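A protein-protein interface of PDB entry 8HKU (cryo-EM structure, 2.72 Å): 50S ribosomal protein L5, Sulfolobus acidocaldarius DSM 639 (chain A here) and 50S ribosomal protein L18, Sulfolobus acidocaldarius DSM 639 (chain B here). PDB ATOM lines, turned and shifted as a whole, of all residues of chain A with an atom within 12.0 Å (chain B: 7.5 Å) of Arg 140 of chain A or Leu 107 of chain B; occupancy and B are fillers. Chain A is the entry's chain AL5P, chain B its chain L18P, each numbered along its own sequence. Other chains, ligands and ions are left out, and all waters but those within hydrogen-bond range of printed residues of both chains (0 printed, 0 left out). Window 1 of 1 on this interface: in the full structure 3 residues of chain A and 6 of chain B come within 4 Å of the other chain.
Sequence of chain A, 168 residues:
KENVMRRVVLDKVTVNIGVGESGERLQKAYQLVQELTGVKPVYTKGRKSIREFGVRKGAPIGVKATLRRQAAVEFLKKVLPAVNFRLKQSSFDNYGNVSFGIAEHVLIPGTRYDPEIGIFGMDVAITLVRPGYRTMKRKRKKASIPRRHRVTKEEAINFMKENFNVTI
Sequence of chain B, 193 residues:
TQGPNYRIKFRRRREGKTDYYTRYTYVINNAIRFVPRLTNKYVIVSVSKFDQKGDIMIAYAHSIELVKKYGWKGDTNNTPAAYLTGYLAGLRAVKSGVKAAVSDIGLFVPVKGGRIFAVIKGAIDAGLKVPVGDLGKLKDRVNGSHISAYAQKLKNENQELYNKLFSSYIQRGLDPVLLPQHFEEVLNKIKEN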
ATOM      1  N   GLY A 132      23.844  -2.555 -28.916  1.00  0.00           N
ATOM      2  CA  GLY A 132      22.892  -3.581 -28.560  1.00  0.00           C
ATOM      3  C   GLY A 132      22.988  -4.096 -27.144  1.00  0.00           C
ATOM      4  O   GLY A 132      22.231  -5.001 -26.787  1.00  0.00           O
ATOM      5  N   TYR A 133      23.884  -3.547 -26.321  1.00  0.00           N
ATOM      6  CA  TYR A 133      23.994  -3.977 -24.932  1.00  0.00           C
ATOM      7  C   TYR A 133      22.795  -3.563 -24.096  1.00  0.00           C
ATOM      8  O   TYR A 133      22.699  -3.978 -22.938  1.00  0.00           O
ATOM      9  CB  TYR A 133      25.253  -3.413 -24.284  1.00  0.00           C
ATOM     10  CG  TYR A 133      26.488  -4.265 -24.426  1.00  0.00           C
ATOM     11  CD1 TYR A 133      26.739  -4.978 -25.586  1.00  0.00           C
ATOM     12  CD2 TYR A 133      27.406  -4.353 -23.394  1.00  0.00           C
ATOM     13  CE1 TYR A 133      27.876  -5.750 -25.715  1.00  0.00           C
ATOM     14  CE2 TYR A 133      28.542  -5.120 -23.513  1.00  0.00           C
ATOM     15  CZ  TYR A 133      28.772  -5.816 -24.672  1.00  0.00           C
ATOM     16  OH  TYR A 133      29.907  -6.581 -24.784  1.00  0.00           O
ATOM     17  N   ARG A 134      21.898  -2.744 -24.642  1.00  0.00           N
ATOM     18  CA  ARG A 134      20.723  -2.320 -23.897  1.00  0.00           C
ATOM     19  C   ARG A 134      19.856  -3.492 -23.468  1.00  0.00           C
ATOM     20  O   ARG A 134      19.094  -3.364 -22.508  1.00  0.00           O
ATOM     21  CB  ARG A 134      19.895  -1.351 -24.737  1.00  0.00           C
ATOM     22  CG  ARG A 134      18.813  -0.684 -23.954  1.00  0.00           C
ATOM     23  CD  ARG A 134      18.033   0.303 -24.759  1.00  0.00           C
ATOM     24  NE  ARG A 134      17.115   1.017 -23.885  1.00  0.00           N
ATOM     25  CZ  ARG A 134      15.850   0.679 -23.695  1.00  0.00           C
ATOM     26  NH1 ARG A 134      15.292  -0.309 -24.369  1.00  0.00           N
ATOM     27  NH2 ARG A 134      15.127   1.355 -22.814  1.00  0.00           N
ATOM     28  N   THR A 135      19.956  -4.633 -24.147  1.00  0.00           N
ATOM     29  CA  THR A 135      19.088  -5.757 -23.829  1.00  0.00           C
ATOM     30  C   THR A 135      19.356  -6.335 -22.448  1.00  0.00           C
ATOM     31  O   THR A 135      18.478  -6.995 -21.891  1.00  0.00           O
ATOM     32  CB  THR A 135      19.234  -6.848 -24.886  1.00  0.00           C
ATOM     33  OG1 THR A 135      20.586  -7.315 -24.905  1.00  0.00           O
ATOM     34  CG2 THR A 135      18.887  -6.298 -26.248  1.00  0.00           C
ATOM     35  N   MET A 136      20.536  -6.105 -21.879  1.00  0.00           N
ATOM     36  CA  MET A 136      20.822  -6.603 -20.543  1.00  0.00           C
ATOM     37  C   MET A 136      20.407  -5.645 -19.441  1.00  0.00           C
ATOM     38  O   MET A 136      20.258  -6.076 -18.294  1.00  0.00           O
ATOM     39  CB  MET A 136      22.311  -6.897 -20.371  1.00  0.00           C
ATOM     40  CG  MET A 136      22.844  -8.025 -21.205  1.00  0.00           C
ATOM     41  SD  MET A 136      24.585  -8.291 -20.839  1.00  0.00           S
ATOM     42  CE  MET A 136      25.312  -6.881 -21.659  1.00  0.00           C
ATOM     43  N   LYS A 137      20.228  -4.364 -19.746  1.00  0.00           N
ATOM     44  CA  LYS A 137      20.031  -3.361 -18.717  1.00  0.00           C
ATOM     45  C   LYS A 137      18.707  -2.625 -18.817  1.00  0.00           C
ATOM     46  O   LYS A 137      18.412  -1.802 -17.946  1.00  0.00           O
ATOM     47  CB  LYS A 137      21.181  -2.353 -18.747  1.00  0.00           C
ATOM     48  CG  LYS A 137      22.531  -2.988 -18.530  1.00  0.00           C
ATOM     49  CD  LYS A 137      23.629  -1.953 -18.488  1.00  0.00           C
ATOM     50  CE  LYS A 137      24.979  -2.600 -18.222  1.00  0.00           C
ATOM     51  NZ  LYS A 137      25.031  -3.260 -16.892  1.00  0.00           N
ATOM     52  N   ARG A 138      17.901  -2.892 -19.835  1.00  0.00           N
ATOM     53  CA  ARG A 138      16.596  -2.263 -19.898  1.00  0.00           C
ATOM     54  C   ARG A 138      15.648  -2.913 -18.896  1.00  0.00           C
ATOM     55  O   ARG A 138      15.938  -3.953 -18.304  1.00  0.00           O
ATOM     56  CB  ARG A 138      16.032  -2.341 -21.311  1.00  0.00           C
ATOM     57  CG  ARG A 138      15.786  -3.741 -21.786  1.00  0.00           C
ATOM     58  CD  ARG A 138      15.464  -3.770 -23.254  1.00  0.00           C
ATOM     59  NE  ARG A 138      15.110  -5.110 -23.692  1.00  0.00           N
ATOM     60  CZ  ARG A 138      15.133  -5.519 -24.951  1.00  0.00           C
ATOM     61  NH1 ARG A 138      15.501  -4.714 -25.931  1.00  0.00           N
ATOM     62  NH2 ARG A 138      14.783  -6.768 -25.234  1.00  0.00           N
ATOM     63  N   LYS A 139      14.500  -2.274 -18.696  1.00  0.00           N
ATOM     64  CA  LYS A 139      13.570  -2.729 -17.671  1.00  0.00           C
ATOM     65  C   LYS A 139      12.647  -3.825 -18.183  1.00  0.00           C
ATOM     66  O   LYS A 139      12.442  -4.836 -17.506  1.00  0.00           O
ATOM     67  CB  LYS A 139      12.752  -1.551 -17.150  1.00  0.00           C
ATOM     68  CG  LYS A 139      11.638  -1.961 -16.226  1.00  0.00           C
ATOM     69  CD  LYS A 139      11.133  -0.800 -15.406  1.00  0.00           C
ATOM     70  CE  LYS A 139      10.117  -1.274 -14.395  1.00  0.00           C
ATOM     71  NZ  LYS A 139       9.938  -0.300 -13.300  1.00  0.00           N
ATOM     72  N   ARG A 140      12.077  -3.645 -19.365  1.00  0.00           N
ATOM     73  CA  ARG A 140      11.103  -4.577 -19.906  1.00  0.00           C
ATOM     74  C   ARG A 140      11.754  -5.488 -20.934  1.00  0.00           C
ATOM     75  O   ARG A 140      12.578  -5.045 -21.735  1.00  0.00           O
ATOM     76  CB  ARG A 140       9.932  -3.832 -20.542  1.00  0.00           C
ATOM     77  CG  ARG A 140       9.124  -3.017 -19.565  1.00  0.00           C
ATOM     78  CD  ARG A 140       8.135  -2.130 -20.275  1.00  0.00           C
ATOM     79  NE  ARG A 140       8.795  -1.031 -20.966  1.00  0.00           N
ATOM     80  CZ  ARG A 140       9.165   0.102 -20.389  1.00  0.00           C
ATOM     81  NH1 ARG A 140       8.947   0.330 -19.107  1.00  0.00           N
ATOM     82  NH2 ARG A 140       9.771   1.032 -21.118  1.00  0.00           N
ATOM     83  N   LYS A 141      11.375  -6.765 -20.897  1.00  0.00           N
ATOM     84  CA  LYS A 141      11.850  -7.773 -21.842  1.00  0.00           C
ATOM     85  C   LYS A 141      13.370  -7.861 -21.863  1.00  0.00           C
ATOM     86  O   LYS A 141      13.978  -8.024 -22.919  1.00  0.00           O
ATOM     87  CB  LYS A 141      11.321  -7.512 -23.250  1.00  0.00           C
ATOM     88  CG  LYS A 141       9.844  -7.252 -23.334  1.00  0.00           C
ATOM     89  CD  LYS A 141       9.415  -7.116 -24.774  1.00  0.00           C
ATOM     90  CE  LYS A 141       8.114  -6.351 -24.887  1.00  0.00           C
ATOM     91  NZ  LYS A 141       6.999  -7.037 -24.183  1.00  0.00           N
ATOM     92  N   LYS A 142      13.997  -7.750 -20.699  1.00  0.00           N
ATOM     93  CA  LYS A 142      15.446  -7.826 -20.666  1.00  0.00           C
ATOM     94  C   LYS A 142      15.900  -9.260 -20.894  1.00  0.00           C
ATOM     95  O   LYS A 142      15.210 -10.220 -20.542  1.00  0.00           O
ATOM     96  CB  LYS A 142      15.993  -7.291 -19.349  1.00  0.00           C
ATOM     97  CG  LYS A 142      15.816  -8.200 -18.176  1.00  0.00           C
ATOM     98  CD  LYS A 142      16.056  -7.448 -16.891  1.00  0.00           C
ATOM     99  CE  LYS A 142      17.458  -6.901 -16.836  1.00  0.00           C
ATOM    100  NZ  LYS A 142      17.656  -6.084 -15.611  1.00  0.00           N
ATOM    101  N   ALA A 143      17.068  -9.401 -21.510  1.00  0.00           N
ATOM    102  CA  ALA A 143      17.561 -10.691 -21.957  1.00  0.00           C
ATOM    103  C   ALA A 143      19.057 -10.747 -21.695  1.00  0.00           C
ATOM    104  O   ALA A 143      19.603  -9.950 -20.928  1.00  0.00           O
ATOM    105  CB  ALA A 143      17.220 -10.915 -23.433  1.00  0.00           C
ATOM    106  N   SER A 144      19.725 -11.708 -22.321  1.00  0.00           N
ATOM    107  CA  SER A 144      21.165 -11.854 -22.201  1.00  0.00           C
ATOM    108  C   SER A 144      21.779 -11.967 -23.588  1.00  0.00           C
ATOM    109  O   SER A 144      21.134 -12.426 -24.533  1.00  0.00           O
ATOM    110  CB  SER A 144      21.537 -13.075 -21.361  1.00  0.00           C
ATOM    111  OG  SER A 144      22.912 -13.055 -21.028  1.00  0.00           O
ATOM    112  N   ARG B  12       5.875 -16.082 -19.310  1.00  0.00           N
ATOM    113  CA  ARG B  12       5.857 -14.637 -19.477  1.00  0.00           C
ATOM    114  C   ARG B  12       6.746 -13.924 -18.469  1.00  0.00           C
ATOM    115  O   ARG B  12       7.140 -12.784 -18.711  1.00  0.00           O
ATOM    116  CB  ARG B  12       4.430 -14.116 -19.362  1.00  0.00           C
ATOM    117  CG  ARG B  12       3.445 -14.792 -20.280  1.00  0.00           C
ATOM    118  CD  ARG B  12       3.352 -14.072 -21.581  1.00  0.00           C
ATOM    119  NE  ARG B  12       2.444 -12.938 -21.502  1.00  0.00           N
ATOM    120  CZ  ARG B  12       2.302 -12.033 -22.457  1.00  0.00           C
ATOM    121  NH1 ARG B  12       2.997 -12.099 -23.577  1.00  0.00           N
ATOM    122  NH2 ARG B  12       1.442 -11.039 -22.284  1.00  0.00           N
ATOM    123  N   ARG B  13       7.059 -14.554 -17.341  1.00  0.00           N
ATOM    124  CA  ARG B  13       8.024 -13.967 -16.421  1.00  0.00           C
ATOM    125  C   ARG B  13       9.444 -14.140 -16.938  1.00  0.00           C
ATOM    126  O   ARG B  13      10.287 -13.256 -16.764  1.00  0.00           O
ATOM    127  CB  ARG B  13       7.870 -14.586 -15.034  1.00  0.00           C
ATOM    128  CG  ARG B  13       8.984 -14.259 -14.063  1.00  0.00           C
ATOM    129  CD  ARG B  13       9.031 -12.794 -13.718  1.00  0.00           C
ATOM    130  NE  ARG B  13      10.153 -12.493 -12.841  1.00  0.00           N
ATOM    131  CZ  ARG B  13      11.318 -12.018 -13.252  1.00  0.00           C
ATOM    132  NH1 ARG B  13      11.536 -11.731 -14.521  1.00  0.00           N
ATOM    133  NH2 ARG B  13      12.286 -11.821 -12.366  1.00  0.00           N
ATOM    134  N   GLU B  15      10.267 -14.248 -20.130  1.00  0.00           N
ATOM    135  CA  GLU B  15      10.367 -13.296 -21.225  1.00  0.00           C
ATOM    136  C   GLU B  15      10.357 -11.850 -20.761  1.00  0.00           C
ATOM    137  O   GLU B  15      10.585 -10.958 -21.580  1.00  0.00           O
ATOM    138  CB  GLU B  15       9.228 -13.517 -22.213  1.00  0.00           C
ATOM    139  CG  GLU B  15       9.163 -14.920 -22.755  1.00  0.00           C
ATOM    140  CD  GLU B  15       7.922 -15.165 -23.578  1.00  0.00           C
ATOM    141  OE1 GLU B  15       6.918 -14.457 -23.374  1.00  0.00           O
ATOM    142  OE2 GLU B  15       7.950 -16.075 -24.430  1.00  0.00           O
ATOM    143  N   GLY B  16      10.108 -11.599 -19.481  1.00  0.00           N
ATOM    144  CA  GLY B  16      10.033 -10.251 -18.953  1.00  0.00           C
ATOM    145  C   GLY B  16       8.844  -9.449 -19.429  1.00  0.00           C
ATOM    146  O   GLY B  16       8.982  -8.253 -19.696  1.00  0.00           O
ATOM    147  N   LYS B  17       7.672 -10.066 -19.514  1.00  0.00           N
ATOM    148  CA  LYS B  17       6.493  -9.411 -20.064  1.00  0.00           C
ATOM    149  C   LYS B  17       5.381  -9.167 -19.056  1.00  0.00           C
ATOM    150  O   LYS B  17       4.726  -8.127 -19.117  1.00  0.00           O
ATOM    151  CB  LYS B  17       5.936 -10.235 -21.223  1.00  0.00           C
ATOM    152  CG  LYS B  17       6.697 -10.089 -22.519  1.00  0.00           C
ATOM    153  CD  LYS B  17       5.909 -10.720 -23.644  1.00  0.00           C
ATOM    154  CE  LYS B  17       6.566 -10.525 -24.985  1.00  0.00           C
ATOM    155  NZ  LYS B  17       7.942 -11.066 -24.999  1.00  0.00           N
ATOM    156  N   THR B  18       5.130 -10.092 -18.135  1.00  0.00           N
ATOM    157  CA  THR B  18       3.996 -10.003 -17.224  1.00  0.00           C
ATOM    158  C   THR B  18       4.475  -9.939 -15.782  1.00  0.00           C
ATOM    159  O   THR B  18       5.459 -10.585 -15.413  1.00  0.00           O
ATOM    160  CB  THR B  18       3.053 -11.190 -17.400  1.00  0.00           C
ATOM    161  OG1 THR B  18       2.755 -11.352 -18.787  1.00  0.00           O
ATOM    162  CG2 THR B  18       1.762 -10.965 -16.658  1.00  0.00           C
ATOM    163  N   ASP B  19       3.781  -9.136 -14.975  1.00  0.00           N
ATOM    164  CA  ASP B  19       4.015  -9.042 -13.537  1.00  0.00           C
ATOM    165  C   ASP B  19       2.882  -9.783 -12.842  1.00  0.00           C
ATOM    166  O   ASP B  19       1.770  -9.269 -12.729  1.00  0.00           O
ATOM    167  CB  ASP B  19       4.091  -7.587 -13.096  1.00  0.00           C
ATOM    168  CG  ASP B  19       4.261  -7.437 -11.602  1.00  0.00           C
ATOM    169  OD1 ASP B  19       5.354  -7.734 -11.085  1.00  0.00           O
ATOM    170  OD2 ASP B  19       3.302  -7.006 -10.938  1.00  0.00           O
ATOM    171  N   ARG B  37      -0.832  -0.323 -23.603  1.00  0.00           N
ATOM    172  CA  ARG B  37       0.550  -0.672 -23.910  1.00  0.00           C
ATOM    173  C   ARG B  37       1.167   0.302 -24.913  1.00  0.00           C
ATOM    174  O   ARG B  37       0.472   1.036 -25.611  1.00  0.00           O
ATOM    175  CB  ARG B  37       0.633  -2.094 -24.453  1.00  0.00           C
ATOM    176  CG  ARG B  37       0.435  -3.155 -23.404  1.00  0.00           C
ATOM    177  CD  ARG B  37       1.391  -2.992 -22.248  1.00  0.00           C
ATOM    178  NE  ARG B  37       1.090  -3.950 -21.194  1.00  0.00           N
ATOM    179  CZ  ARG B  37       0.372  -3.681 -20.115  1.00  0.00           C
ATOM    180  NH1 ARG B  37      -0.106  -2.472 -19.887  1.00  0.00           N
ATOM    181  NH2 ARG B  37       0.121  -4.652 -19.246  1.00  0.00           N
ATOM    182  N   LEU B  38       2.499   0.286 -24.980  1.00  0.00           N
ATOM    183  CA  LEU B  38       3.275   1.128 -25.882  1.00  0.00           C
ATOM    184  C   LEU B  38       4.395   0.314 -26.518  1.00  0.00           C
ATOM    185  O   LEU B  38       4.834  -0.701 -25.977  1.00  0.00           O
ATOM    186  CB  LEU B  38       3.895   2.326 -25.154  1.00  0.00           C
ATOM    187  CG  LEU B  38       3.082   3.591 -24.891  1.00  0.00           C
ATOM    188  CD1 LEU B  38       3.817   4.453 -23.892  1.00  0.00           C
ATOM    189  CD2 LEU B  38       2.839   4.362 -26.164  1.00  0.00           C
ATOM    190  N   ASP B 104      -4.530  -0.869 -16.137  1.00  0.00           N
ATOM    191  CA  ASP B 104      -3.493  -1.899 -16.041  1.00  0.00           C
ATOM    192  C   ASP B 104      -2.227  -1.361 -16.703  1.00  0.00           C
ATOM    193  O   ASP B 104      -2.041  -1.510 -17.910  1.00  0.00           O
ATOM    194  CB  ASP B 104      -3.950  -3.185 -16.704  1.00  0.00           C
ATOM    195  CG  ASP B 104      -3.097  -4.374 -16.324  1.00  0.00           C
ATOM    196  OD1 ASP B 104      -1.876  -4.205 -16.135  1.00  0.00           O
ATOM    197  OD2 ASP B 104      -3.645  -5.491 -16.249  1.00  0.00           O
ATOM    198  N   ILE B 105      -1.346  -0.754 -15.912  1.00  0.00           N
ATOM    199  CA  ILE B 105      -0.139  -0.157 -16.476  1.00  0.00           C
ATOM    200  C   ILE B 105       0.814  -1.227 -16.980  1.00  0.00           C
ATOM    201  O   ILE B 105       1.446  -1.066 -18.028  1.00  0.00           O
ATOM    202  CB  ILE B 105       0.531   0.766 -15.444  1.00  0.00           C
ATOM    203  CG1 ILE B 105      -0.427   1.871 -15.031  1.00  0.00           C
ATOM    204  CG2 ILE B 105       1.795   1.359 -15.976  1.00  0.00           C
ATOM    205  CD1 ILE B 105      -1.228   2.441 -16.159  1.00  0.00           C
ATOM    206  N   GLY B 106       0.943  -2.322 -16.255  1.00  0.00           N
ATOM    207  CA  GLY B 106       1.875  -3.369 -16.633  1.00  0.00           C
ATOM    208  C   GLY B 106       3.225  -3.148 -15.991  1.00  0.00           C
ATOM    209  O   GLY B 106       3.318  -2.973 -14.782  1.00  0.00           O
ATOM    210  N   LEU B 107       4.275  -3.159 -16.805  1.00  0.00           N
ATOM    211  CA  LEU B 107       5.627  -2.917 -16.330  1.00  0.00           C
ATOM    212  C   LEU B 107       6.129  -1.521 -16.659  1.00  0.00           C
ATOM    213  O   LEU B 107       7.332  -1.267 -16.554  1.00  0.00           O
ATOM    214  CB  LEU B 107       6.582  -3.963 -16.901  1.00  0.00           C
ATOM    215  CG  LEU B 107       6.697  -5.275 -16.131  1.00  0.00           C
ATOM    216  CD1 LEU B 107       7.533  -6.254 -16.906  1.00  0.00           C
ATOM    217  CD2 LEU B 107       7.316  -5.012 -14.782  1.00  0.00           C
ATOM    218  N   PHE B 108       5.246  -0.614 -17.058  1.00  0.00           N
ATOM    219  CA  PHE B 108       5.634   0.766 -17.298  1.00  0.00           C
ATOM    220  C   PHE B 108       5.636   1.556 -15.998  1.00  0.00           C
ATOM    221  O   PHE B 108       4.933   1.223 -15.044  1.00  0.00           O
ATOM    222  CB  PHE B 108       4.691   1.423 -18.300  1.00  0.00           C
ATOM    223  CG  PHE B 108       4.818   0.885 -19.690  1.00  0.00           C
ATOM    224  CD1 PHE B 108       5.778   1.378 -20.547  1.00  0.00           C
ATOM    225  CD2 PHE B 108       3.979  -0.112 -20.140  1.00  0.00           C
ATOM    226  CE1 PHE B 108       5.895   0.887 -21.821  1.00  0.00           C
ATOM    227  CE2 PHE B 108       4.099  -0.607 -21.414  1.00  0.00           C
ATOM    228  CZ  PHE B 108       5.058  -0.105 -22.254  1.00  0.00           C
ATOM    229  N   VAL B 109       6.439   2.613 -15.967  1.00  0.00           N
ATOM    230  CA  VAL B 109       6.555   3.468 -14.789  1.00  0.00           C
ATOM    231  C   VAL B 109       5.500   4.565 -14.849  1.00  0.00           C
ATOM    232  O   VAL B 109       5.419   5.290 -15.848  1.00  0.00           O
ATOM    233  CB  VAL B 109       7.964   4.063 -14.675  1.00  0.00           C
ATOM    234  CG1 VAL B 109       8.058   4.945 -13.462  1.00  0.00           C
ATOM    235  CG2 VAL B 109       8.992   2.959 -14.605  1.00  0.00           C
ATOM    236  N   PRO B 110       4.670   4.720 -13.819  1.00  0.00           N
ATOM    237  CA  PRO B 110       3.609   5.735 -13.865  1.00  0.00           C
ATOM    238  C   PRO B 110       4.107   7.139 -13.562  1.00  0.00           C
ATOM    239  O   PRO B 110       4.083   7.581 -12.411  1.00  0.00           O
ATOM    240  CB  PRO B 110       2.624   5.247 -12.800  1.00  0.00           C
ATOM    241  CG  PRO B 110       3.473   4.532 -11.831  1.00  0.00           C
ATOM    242  CD  PRO B 110       4.598   3.908 -12.594  1.00  0.00           C
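N of Lys 141 of chain A lies within hydrogen-bond range of O of Gly 16 of chain B (3.1 Å). The backbone carbonyl oxygen of Leu 107 of chain B sits at hydrogen-bond distance from the guanidinium group of Arg 140 of chain A, at 3.4 Å.
O of Arg 12 of chain B lies within hydrogen-bond range of N of Lys 17 of chain B. OE1 of Glu 15 of chain B is in salt-bridge range of NZ of Lys 17 of chain B. The guanidinium group (NE) of Arg 138 of chain A is in hydrogen-bond range of the backbone carbonyl oxygen (O) of Arg 140 of chain A, at 3.2 Å. The backbone carbonyl oxygen of Lys 141 of chain A is in hydrogen-bond range of the guanidinium group of Arg 138 of chain A, at 2.8 Å.
Lys 139 of chain A touches Leu 107 of chain B. NZ of Lys 139 of chain A touches CG2 of Val 109 of chain B (3.6 Å). NE of Arg 140 of chain A touches CE1 of Phe 108 of chain B, at 3.6 Å. CA of Lys 141 of chain A touches O of Glu 15 of chain B, 3.4 Å away. CG of Lys 17 of chain B touches NZ of Lys 141 of chain A (3.5 Å).
Of the printed residues of chain B, Lys 139 of chain A touches Leu 107 and Val 109. Arg 140 of chain A touches just these residues of chain B: Leu 107 (3.4 Å) and Phe 108 (3.6 Å). Printed residues of chain B within 4 Å of Lys 141 of chain A: Glu 15 (3.4 Å), Gly 16 (3.1 Å) and Lys 17 (3.5 Å). Ser 144 of chain A touches none of the printed residues of chain B. Of the printed residues of chain A, Glu 15 of chain B touches Lys 141. Printed residues of chain A within 4 Å of Gly 16 of chain B: Lys 141 (3.1 Å). Of the printed residues of chain A, Lys 17 of chain B touches Lys 141. No residue of chain A comes within 4 Å of Thr 18 of chain B. No residue of chain A comes within 4 Å of Asp 19 of chain B. No residue of chain A comes within 4 Å of Ile 105 of chain B. Gly 106 of chain B touches none of the printed residues of chain A. Leu 107 of chain B touches two residues of chain A. Val 109 of chain B touches just one residue of chain A: Lys 139. The nearest residue of chain B that does not touch Arg 140 of chain A is Gly 16 of chain B (4.1 Å). The nearest residue of chain A that does not touch Leu 107 of chain B is Lys 141 of chain A (5.6 Å). The nearest printed residue of chain A that does not touch Lys 17 of chain B is Arg 140 of chain A (6.3 Å).
Of the 16 printed residues of chain B, 6 touch a printed residue of chain A. Printed residues of chain B that touch a printed residue of chain A: Glu 15, Gly 16, Lys 17, Leu 107, Phe 108 and Val 109. Of the 13 printed residues of chain A, 3 touch a printed residue of chain B. Among the printed residues, 7 pairs touch across the chains. Among the printed residues, no Asp or Glu carboxylate lies within 4 Å of a Lys or Arg side-chain nitrogen of the other chain.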
